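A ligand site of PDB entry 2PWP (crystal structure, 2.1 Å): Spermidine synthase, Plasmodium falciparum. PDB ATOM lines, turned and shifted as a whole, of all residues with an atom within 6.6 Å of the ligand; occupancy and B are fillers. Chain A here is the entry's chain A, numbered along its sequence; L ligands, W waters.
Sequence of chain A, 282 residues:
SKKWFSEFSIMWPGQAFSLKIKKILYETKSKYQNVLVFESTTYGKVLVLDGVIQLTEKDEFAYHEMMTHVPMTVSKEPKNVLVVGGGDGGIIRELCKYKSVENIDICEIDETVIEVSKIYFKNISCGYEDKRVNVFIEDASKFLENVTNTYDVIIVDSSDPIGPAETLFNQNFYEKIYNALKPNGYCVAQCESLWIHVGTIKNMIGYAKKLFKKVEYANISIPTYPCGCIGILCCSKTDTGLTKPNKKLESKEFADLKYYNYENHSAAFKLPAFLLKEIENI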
ATOM      1  N   GLU A   7       5.566   6.636   5.416  1.00  0.00           N
ATOM      2  CA  GLU A   7       4.561   7.205   6.298  1.00  0.00           C
ATOM      3  C   GLU A   7       5.043   7.227   7.752  1.00  0.00           C
ATOM      4  O   GLU A   7       4.991   6.220   8.454  1.00  0.00           O
ATOM      5  CB  GLU A   7       3.250   6.418   6.180  1.00  0.00           C
ATOM      6  CG  GLU A   7       2.052   7.051   6.844  1.00  0.00           C
ATOM      7  CD  GLU A   7       0.872   6.104   6.945  1.00  0.00           C
ATOM      8  OE1 GLU A   7       1.074   4.944   7.363  1.00  0.00           O
ATOM      9  OE2 GLU A   7      -0.265   6.500   6.604  1.00  0.00           O
ATOM     10  N   MET A  11       2.018   9.665  15.997  1.00  0.00           N
ATOM     11  CA  MET A  11       0.898   8.800  16.379  1.00  0.00           C
ATOM     12  C   MET A  11       1.276   7.314  16.304  1.00  0.00           C
ATOM     13  O   MET A  11       0.581   6.459  16.857  1.00  0.00           O
ATOM     14  CB  MET A  11      -0.309   9.073  15.480  1.00  0.00           C
ATOM     15  CG  MET A  11      -0.909  10.464  15.632  1.00  0.00           C
ATOM     16  SD  MET A  11      -2.420  10.682  14.665  1.00  0.00           S
ATOM     17  CE  MET A  11      -1.765  10.788  13.000  1.00  0.00           C
ATOM     18  N   TRP A  12       2.363   6.994  15.606  1.00  0.00           N
ATOM     19  CA  TRP A  12       2.898   5.637  15.627  1.00  0.00           C
ATOM     20  C   TRP A  12       4.430   5.645  15.539  1.00  0.00           C
ATOM     21  O   TRP A  12       5.018   5.280  14.516  1.00  0.00           O
ATOM     22  CB  TRP A  12       2.274   4.746  14.551  1.00  0.00           C
ATOM     23  CG  TRP A  12       2.136   5.361  13.181  1.00  0.00           C
ATOM     24  CD1 TRP A  12       3.079   5.378  12.188  1.00  0.00           C
ATOM     25  CD2 TRP A  12       0.976   6.004  12.638  1.00  0.00           C
ATOM     26  NE1 TRP A  12       2.578   6.015  11.075  1.00  0.00           N
ATOM     27  CE2 TRP A  12       1.297   6.405  11.325  1.00  0.00           C
ATOM     28  CE3 TRP A  12      -0.297   6.295  13.150  1.00  0.00           C
ATOM     29  CZ2 TRP A  12       0.389   7.079  10.513  1.00  0.00           C
ATOM     30  CZ3 TRP A  12      -1.192   6.966  12.334  1.00  0.00           C
ATOM     31  CH2 TRP A  12      -0.848   7.355  11.036  1.00  0.00           C
ATOM     32  N   VAL A  52      -0.094  11.291   5.679  1.00  0.00           N
ATOM     33  CA  VAL A  52      -0.778  10.089   6.151  1.00  0.00           C
ATOM     34  C   VAL A  52      -1.594   9.490   5.012  1.00  0.00           C
ATOM     35  O   VAL A  52      -2.378  10.182   4.361  1.00  0.00           O
ATOM     36  CB  VAL A  52      -1.692  10.379   7.352  1.00  0.00           C
ATOM     37  CG1 VAL A  52      -2.553   9.172   7.676  1.00  0.00           C
ATOM     38  CG2 VAL A  52      -0.851  10.775   8.554  1.00  0.00           C
ATOM     39  N   ILE A  53      -1.400   8.196   4.773  1.00  0.00           N
ATOM     40  CA  ILE A  53      -2.119   7.504   3.715  1.00  0.00           C
ATOM     41  C   ILE A  53      -3.610   7.432   4.043  1.00  0.00           C
ATOM     42  O   ILE A  53      -3.993   6.922   5.087  1.00  0.00           O
ATOM     43  CB  ILE A  53      -1.579   6.075   3.488  1.00  0.00           C
ATOM     44  CG1 ILE A  53      -0.130   6.105   3.016  1.00  0.00           C
ATOM     45  CG2 ILE A  53      -2.452   5.343   2.485  1.00  0.00           C
ATOM     46  CD1 ILE A  53       0.552   4.746   2.996  1.00  0.00           C
ATOM     47  N   GLN A  54      -4.427   7.950   3.129  1.00  0.00           N
ATOM     48  CA  GLN A  54      -5.879   7.946   3.288  1.00  0.00           C
ATOM     49  C   GLN A  54      -6.485   6.735   2.604  1.00  0.00           C
ATOM     50  O   GLN A  54      -7.442   6.143   3.085  1.00  0.00           O
ATOM     51  CB  GLN A  54      -6.466   9.208   2.661  1.00  0.00           C
ATOM     52  CG  GLN A  54      -5.898  10.450   3.282  1.00  0.00           C
ATOM     53  CD  GLN A  54      -6.356  10.608   4.703  1.00  0.00           C
ATOM     54  OE1 GLN A  54      -5.538  10.804   5.619  1.00  0.00           O
ATOM     55  NE2 GLN A  54      -7.666  10.505   4.920  1.00  0.00           N
ATOM     56  N   LEU A  55      -5.921   6.371   1.463  1.00  0.00           N
ATOM     57  CA  LEU A  55      -6.417   5.206   0.757  1.00  0.00           C
ATOM     58  C   LEU A  55      -5.497   4.841  -0.380  1.00  0.00           C
ATOM     59  O   LEU A  55      -4.702   5.662  -0.836  1.00  0.00           O
ATOM     60  CB  LEU A  55      -7.832   5.462   0.219  1.00  0.00           C
ATOM     61  CG  LEU A  55      -8.092   6.539  -0.834  1.00  0.00           C
ATOM     62  CD1 LEU A  55      -7.767   6.054  -2.246  1.00  0.00           C
ATOM     63  CD2 LEU A  55      -9.540   6.969  -0.767  1.00  0.00           C
ATOM     64  N   GLU A  60      -8.798  -0.142  -0.605  1.00  0.00           N
ATOM     65  CA  GLU A  60      -9.782   0.751   0.019  1.00  0.00           C
ATOM     66  C   GLU A  60     -11.137   0.091   0.178  1.00  0.00           C
ATOM     67  O   GLU A  60     -11.899   0.438   1.074  1.00  0.00           O
ATOM     68  CB  GLU A  60      -9.933   2.090  -0.743  1.00  0.00           C
ATOM     69  CG  GLU A  60     -10.289   1.993  -2.219  1.00  0.00           C
ATOM     70  CD  GLU A  60     -11.760   1.669  -2.499  1.00  0.00           C
ATOM     71  OE1 GLU A  60     -12.630   1.922  -1.631  1.00  0.00           O
ATOM     72  OE2 GLU A  60     -12.037   1.177  -3.617  1.00  0.00           O
ATOM     73  N   TYR A  63     -11.987  -1.067   3.813  1.00  0.00           N
ATOM     74  CA  TYR A  63     -12.416  -0.047   4.754  1.00  0.00           C
ATOM     75  C   TYR A  63     -13.805   0.502   4.425  1.00  0.00           C
ATOM     76  O   TYR A  63     -14.684   0.587   5.282  1.00  0.00           O
ATOM     77  CB  TYR A  63     -11.396   1.094   4.773  1.00  0.00           C
ATOM     78  CG  TYR A  63     -11.811   2.275   5.609  1.00  0.00           C
ATOM     79  CD1 TYR A  63     -11.641   2.251   6.987  1.00  0.00           C
ATOM     80  CD2 TYR A  63     -12.348   3.421   5.026  1.00  0.00           C
ATOM     81  CE1 TYR A  63     -12.001   3.332   7.760  1.00  0.00           C
ATOM     82  CE2 TYR A  63     -12.719   4.506   5.813  1.00  0.00           C
ATOM     83  CZ  TYR A  63     -12.536   4.456   7.177  1.00  0.00           C
ATOM     84  OH  TYR A  63     -12.888   5.516   7.970  1.00  0.00           O
ATOM     85  N   HIS A  64     -14.009   0.889   3.167  1.00  0.00           N
ATOM     86  CA  HIS A  64     -15.278   1.484   2.771  1.00  0.00           C
ATOM     87  C   HIS A  64     -16.474   0.505   2.868  1.00  0.00           C
ATOM     88  O   HIS A  64     -17.510   0.862   3.414  1.00  0.00           O
ATOM     89  CB  HIS A  64     -15.149   2.155   1.386  1.00  0.00           C
ATOM     90  CG  HIS A  64     -14.175   3.296   1.376  1.00  0.00           C
ATOM     91  ND1 HIS A  64     -13.133   3.382   0.487  1.00  0.00           N
ATOM     92  CD2 HIS A  64     -14.085   4.395   2.178  1.00  0.00           C
ATOM     93  CE1 HIS A  64     -12.443   4.488   0.714  1.00  0.00           C
ATOM     94  NE2 HIS A  64     -13.001   5.116   1.739  1.00  0.00           N
ATOM     95  N   GLY A  86     -14.595  12.018   4.736  1.00  0.00           N
ATOM     96  CA  GLY A  86     -14.766  11.175   3.561  1.00  0.00           C
ATOM     97  C   GLY A  86     -14.943  11.891   2.230  1.00  0.00           C
ATOM     98  O   GLY A  86     -15.758  11.477   1.395  1.00  0.00           O
ATOM     99  N   GLY A  87     -14.188  12.960   2.035  1.00  0.00           N
ATOM    100  CA  GLY A  87     -14.223  13.694   0.767  1.00  0.00           C
ATOM    101  C   GLY A  87     -13.857  12.821  -0.433  1.00  0.00           C
ATOM    102  O   GLY A  87     -14.208  13.139  -1.554  1.00  0.00           O
ATOM    103  N   ASP A  88     -13.162  11.719  -0.198  1.00  0.00           N
ATOM    104  CA  ASP A  88     -12.756  10.847  -1.305  1.00  0.00           C
ATOM    105  C   ASP A  88     -13.940  10.130  -1.939  1.00  0.00           C
ATOM    106  O   ASP A  88     -13.849   9.696  -3.090  1.00  0.00           O
ATOM    107  CB  ASP A  88     -11.712   9.829  -0.838  1.00  0.00           C
ATOM    108  CG  ASP A  88     -12.191   8.990   0.330  1.00  0.00           C
ATOM    109  OD1 ASP A  88     -13.062   8.110   0.144  1.00  0.00           O
ATOM    110  OD2 ASP A  88     -11.697   9.237   1.449  1.00  0.00           O
ATOM    111  N   GLY A  89     -15.035   9.974  -1.209  1.00  0.00           N
ATOM    112  CA  GLY A  89     -16.250   9.381  -1.768  1.00  0.00           C
ATOM    113  C   GLY A  89     -16.447   7.874  -1.691  1.00  0.00           C
ATOM    114  O   GLY A  89     -17.467   7.349  -2.151  1.00  0.00           O
ATOM    115  N   GLY A  90     -15.490   7.151  -1.098  1.00  0.00           N
ATOM    116  CA  GLY A  90     -15.613   5.711  -0.920  1.00  0.00           C
ATOM    117  C   GLY A  90     -16.847   5.292  -0.150  1.00  0.00           C
ATOM    118  O   GLY A  90     -17.559   4.369  -0.545  1.00  0.00           O
ATOM    119  N   ILE A  91     -17.125   5.969   0.971  1.00  0.00           N
ATOM    120  CA  ILE A  91     -18.353   5.662   1.714  1.00  0.00           C
ATOM    121  C   ILE A  91     -19.559   5.890   0.806  1.00  0.00           C
ATOM    122  O   ILE A  91     -20.401   4.995   0.602  1.00  0.00           O
ATOM    123  CB  ILE A  91     -18.477   6.491   3.013  1.00  0.00           C
ATOM    124  CG1 ILE A  91     -17.240   6.319   3.899  1.00  0.00           C
ATOM    125  CG2 ILE A  91     -19.739   6.101   3.790  1.00  0.00           C
ATOM    126  CD1 ILE A  91     -17.048   4.908   4.404  1.00  0.00           C
ATOM    127  N   ASP A 157     -16.239   9.163   8.822  1.00  0.00           N
ATOM    128  CA  ASP A 157     -15.084   8.718   8.048  1.00  0.00           C
ATOM    129  C   ASP A 157     -13.948   9.698   8.311  1.00  0.00           C
ATOM    130  O   ASP A 157     -13.563  10.490   7.452  1.00  0.00           O
ATOM    131  CB  ASP A 157     -15.467   8.686   6.577  1.00  0.00           C
ATOM    132  CG  ASP A 157     -14.344   8.222   5.698  1.00  0.00           C
ATOM    133  OD1 ASP A 157     -13.340   7.668   6.198  1.00  0.00           O
ATOM    134  OD2 ASP A 157     -14.474   8.414   4.479  1.00  0.00           O
ATOM    135  N   SER A 158     -13.388   9.566   9.500  1.00  0.00           N
ATOM    136  CA  SER A 158     -12.924  10.663  10.322  1.00  0.00           C
ATOM    137  C   SER A 158     -11.621  11.370  10.009  1.00  0.00           C
ATOM    138  O   SER A 158     -11.548  12.591  10.135  1.00  0.00           O
ATOM    139  CB  SER A 158     -12.870  10.185  11.782  1.00  0.00           C
ATOM    140  OG  SER A 158     -11.719  10.670  12.426  1.00  0.00           O
ATOM    141  N   SER A 159     -10.593  10.601   9.627  1.00  0.00           N
ATOM    142  CA  SER A 159      -9.218  11.121   9.562  1.00  0.00           C
ATOM    143  C   SER A 159      -8.584  11.147  10.963  1.00  0.00           C
ATOM    144  O   SER A 159      -9.280  11.309  11.973  1.00  0.00           O
ATOM    145  CB  SER A 159      -9.176  12.505   8.889  1.00  0.00           C
ATOM    146  OG  SER A 159      -7.865  13.033   8.831  1.00  0.00           O
ATOM    147  N   ASP A 160      -7.262  11.000  11.023  1.00  0.00           N
ATOM    148  CA  ASP A 160      -6.527  10.916  12.286  1.00  0.00           C
ATOM    149  C   ASP A 160      -6.639  12.152  13.191  1.00  0.00           C
ATOM    150  O   ASP A 160      -6.799  13.274  12.711  1.00  0.00           O
ATOM    151  CB  ASP A 160      -5.054  10.570  12.032  1.00  0.00           C
ATOM    152  CG  ASP A 160      -4.868   9.141  11.530  1.00  0.00           C
ATOM    153  OD1 ASP A 160      -5.620   8.243  11.966  1.00  0.00           O
ATOM    154  OD2 ASP A 160      -3.957   8.920  10.701  1.00  0.00           O
ATOM    155  N   GLN A 190     -14.553   5.889  12.425  1.00  0.00           N
ATOM    156  CA  GLN A 190     -13.192   5.398  12.344  1.00  0.00           C
ATOM    157  C   GLN A 190     -12.521   5.556  13.697  1.00  0.00           C
ATOM    158  O   GLN A 190     -12.480   6.656  14.263  1.00  0.00           O
ATOM    159  CB  GLN A 190     -12.397   6.155  11.277  1.00  0.00           C
ATOM    160  CG  GLN A 190     -10.997   5.611  11.135  1.00  0.00           C
ATOM    161  CD  GLN A 190     -10.003   6.710  10.903  1.00  0.00           C
ATOM    162  OE1 GLN A 190      -9.174   7.000  11.770  1.00  0.00           O
ATOM    163  NE2 GLN A 190     -10.081   7.348   9.734  1.00  0.00           N
ATOM    164  N   GLU A 192      -9.054   4.176  16.128  1.00  0.00           N
ATOM    165  CA  GLU A 192      -7.679   3.789  15.830  1.00  0.00           C
ATOM    166  C   GLU A 192      -7.355   2.289  15.989  1.00  0.00           C
ATOM    167  O   GLU A 192      -8.170   1.530  16.510  1.00  0.00           O
ATOM    168  CB  GLU A 192      -6.706   4.665  16.622  1.00  0.00           C
ATOM    169  CG  GLU A 192      -6.820   6.159  16.300  1.00  0.00           C
ATOM    170  CD  GLU A 192      -6.564   6.484  14.821  1.00  0.00           C
ATOM    171  OE1 GLU A 192      -5.895   5.682  14.116  1.00  0.00           O
ATOM    172  OE2 GLU A 192      -7.020   7.558  14.354  1.00  0.00           O
ATOM    173  N   THR A 224      -2.680  -1.023   4.240  1.00  0.00           N
ATOM    174  CA  THR A 224      -2.058   0.300   4.093  1.00  0.00           C
ATOM    175  C   THR A 224      -2.436   1.282   5.198  1.00  0.00           C
ATOM    176  O   THR A 224      -2.113   2.455   5.120  1.00  0.00           O
ATOM    177  CB  THR A 224      -2.292   0.920   2.698  1.00  0.00           C
ATOM    178  OG1 THR A 224      -3.691   1.089   2.471  1.00  0.00           O
ATOM    179  CG2 THR A 224      -1.708   0.010   1.616  1.00  0.00           C
ATOM    180  N   TYR A 225      -3.118   0.795   6.232  1.00  0.00           N
ATOM    181  CA  TYR A 225      -3.222   1.575   7.455  1.00  0.00           C
ATOM    182  C   TYR A 225      -2.200   1.049   8.468  1.00  0.00           C
ATOM    183  O   TYR A 225      -1.893  -0.149   8.474  1.00  0.00           O
ATOM    184  CB  TYR A 225      -4.634   1.541   8.040  1.00  0.00           C
ATOM    185  CG  TYR A 225      -5.636   2.387   7.278  1.00  0.00           C
ATOM    186  CD1 TYR A 225      -5.250   3.550   6.632  1.00  0.00           C
ATOM    187  CD2 TYR A 225      -6.976   2.030   7.233  1.00  0.00           C
ATOM    188  CE1 TYR A 225      -6.167   4.333   5.932  1.00  0.00           C
ATOM    189  CE2 TYR A 225      -7.910   2.802   6.538  1.00  0.00           C
ATOM    190  CZ  TYR A 225      -7.498   3.945   5.896  1.00  0.00           C
ATOM    191  OH  TYR A 225      -8.413   4.715   5.217  1.00  0.00           O
ATOM    192  N   PRO A 226      -1.675   1.932   9.323  1.00  0.00           N
ATOM    193  CA  PRO A 226      -0.653   1.550  10.310  1.00  0.00           C
ATOM    194  C   PRO A 226      -1.053   0.302  11.098  1.00  0.00           C
ATOM    195  O   PRO A 226      -2.153   0.223  11.650  1.00  0.00           O
ATOM    196  CB  PRO A 226      -0.581   2.775  11.236  1.00  0.00           C
ATOM    197  CG  PRO A 226      -1.008   3.930  10.351  1.00  0.00           C
ATOM    198  CD  PRO A 226      -2.050   3.360   9.410  1.00  0.00           C
ATOM    199  N   ILE A 230      -7.702  -1.366  11.208  1.00  0.00           N
ATOM    200  CA  ILE A 230      -8.283  -0.172  11.810  1.00  0.00           C
ATOM    201  C   ILE A 230      -9.651  -0.508  12.396  1.00  0.00           C
ATOM    202  O   ILE A 230     -10.333  -1.402  11.918  1.00  0.00           O
ATOM    203  CB  ILE A 230      -8.346   1.036  10.831  1.00  0.00           C
ATOM    204  CG1 ILE A 230      -8.506   2.342  11.601  1.00  0.00           C
ATOM    205  CG2 ILE A 230      -9.439   0.858   9.774  1.00  0.00           C
ATOM    206  CD1 ILE A 230      -7.940   3.538  10.893  1.00  0.00           C
HETATM  207  N1  LIG L   1      -4.389   6.473   9.792  1.00  0.00           N
HETATM  208  C1  LIG L   1      -5.482   6.284   8.829  1.00  0.00           C
HETATM  209  C2  LIG L   1      -6.357   7.538   8.679  1.00  0.00           C
HETATM  210  C3  LIG L   1      -7.431   7.205   7.643  1.00  0.00           C
HETATM  211  C4  LIG L   1      -8.476   8.273   7.237  1.00  0.00           C
HETATM  212  N2  LIG L   1      -9.179   7.506   6.199  1.00  0.00           N
HETATM  213  C5  LIG L   1     -10.153   8.041   5.244  1.00  0.00           C
HETATM  214  C6  LIG L   1     -10.240   6.863   4.248  1.00  0.00           C
HETATM  215  C7  LIG L   1     -11.105   6.998   2.988  1.00  0.00           C
HETATM  216  N3  LIG L   1     -12.504   7.217   3.299  1.00  0.00           N
HETATM  217  O   HOH W   1     -15.119   8.037   2.004  1.00  0.00           O
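The side-chain carboxylate (OD2) of Asp 157 lies within salt-bridge range of a nitrogen (N3) of the ligand (2.6 Å). A nitrogen (N1) of the ligand is in salt-bridge range of the side-chain carboxylate of Asp 160, at 2.6 Å. NE2 of His 64 sits at hydrogen-bond distance from N3 of the ligand (2.7 Å). OD2 of Asp 88 is in salt-bridge range of N3 of the ligand (2.9 Å). OH of Tyr 225 sits close to N2 of the ligand, 3.1 Å away.
OD1 of Asp 157 is in hydrogen-bond range of OH of Tyr 63, at 2.8 Å. O of Asp 157 sits at hydrogen-bond distance from N of Gly 86, 3.3 Å away. NE2 of His 64 lies within hydrogen-bond range of OD1 of Asp 88 (3.4 Å). ND1 of His 64 is in hydrogen-bond range of OE1 of Glu 60, 2.6 Å away. The side-chain hydroxyl of Tyr 225 lies within hydrogen-bond range of the backbone carbonyl oxygen of Gln 54. The side-chain amide nitrogen (NE2) of Gln 190 lies close to the backbone NH (N) of Ser 159 (3.3 Å). The side-chain carboxylate of Glu 192 sits close to the side-chain amide oxygen of Gln 190 (3.4 Å). The side-chain amide oxygen (OE1) of Gln 54 sits close to the backbone carbonyl oxygen (O) of Val 52.
Merely in contact with the ligand: Trp 12, Val 52, Gln 54, Tyr 63, Ser 159, Gln 190 and Pro 226. Hydrophobic or aromatic side chains within 4 Å of the ligand: Trp 12, Val 52, Tyr 63, His 64, Tyr 225 and Pro 226. Within 4 Å of the ligand: Trp 12, Val 52, Gln 54, Tyr 63, His 64, Asp 88, Asp 157, Ser 159, Asp 160, Gln 190, Tyr 225 and Pro 226. The nearest printed residue that does not touch the ligand is Leu 55 (4.1 Å).
Water W1 lies within hydrogen-bond range of OD2 of Asp 157 (2.6 Å), OD1 of Asp 88 (2.8 Å), N3 of the ligand (3.0 Å), N of Ile 91 (3.1 Å) and N of Gly 90 (3.2 Å).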
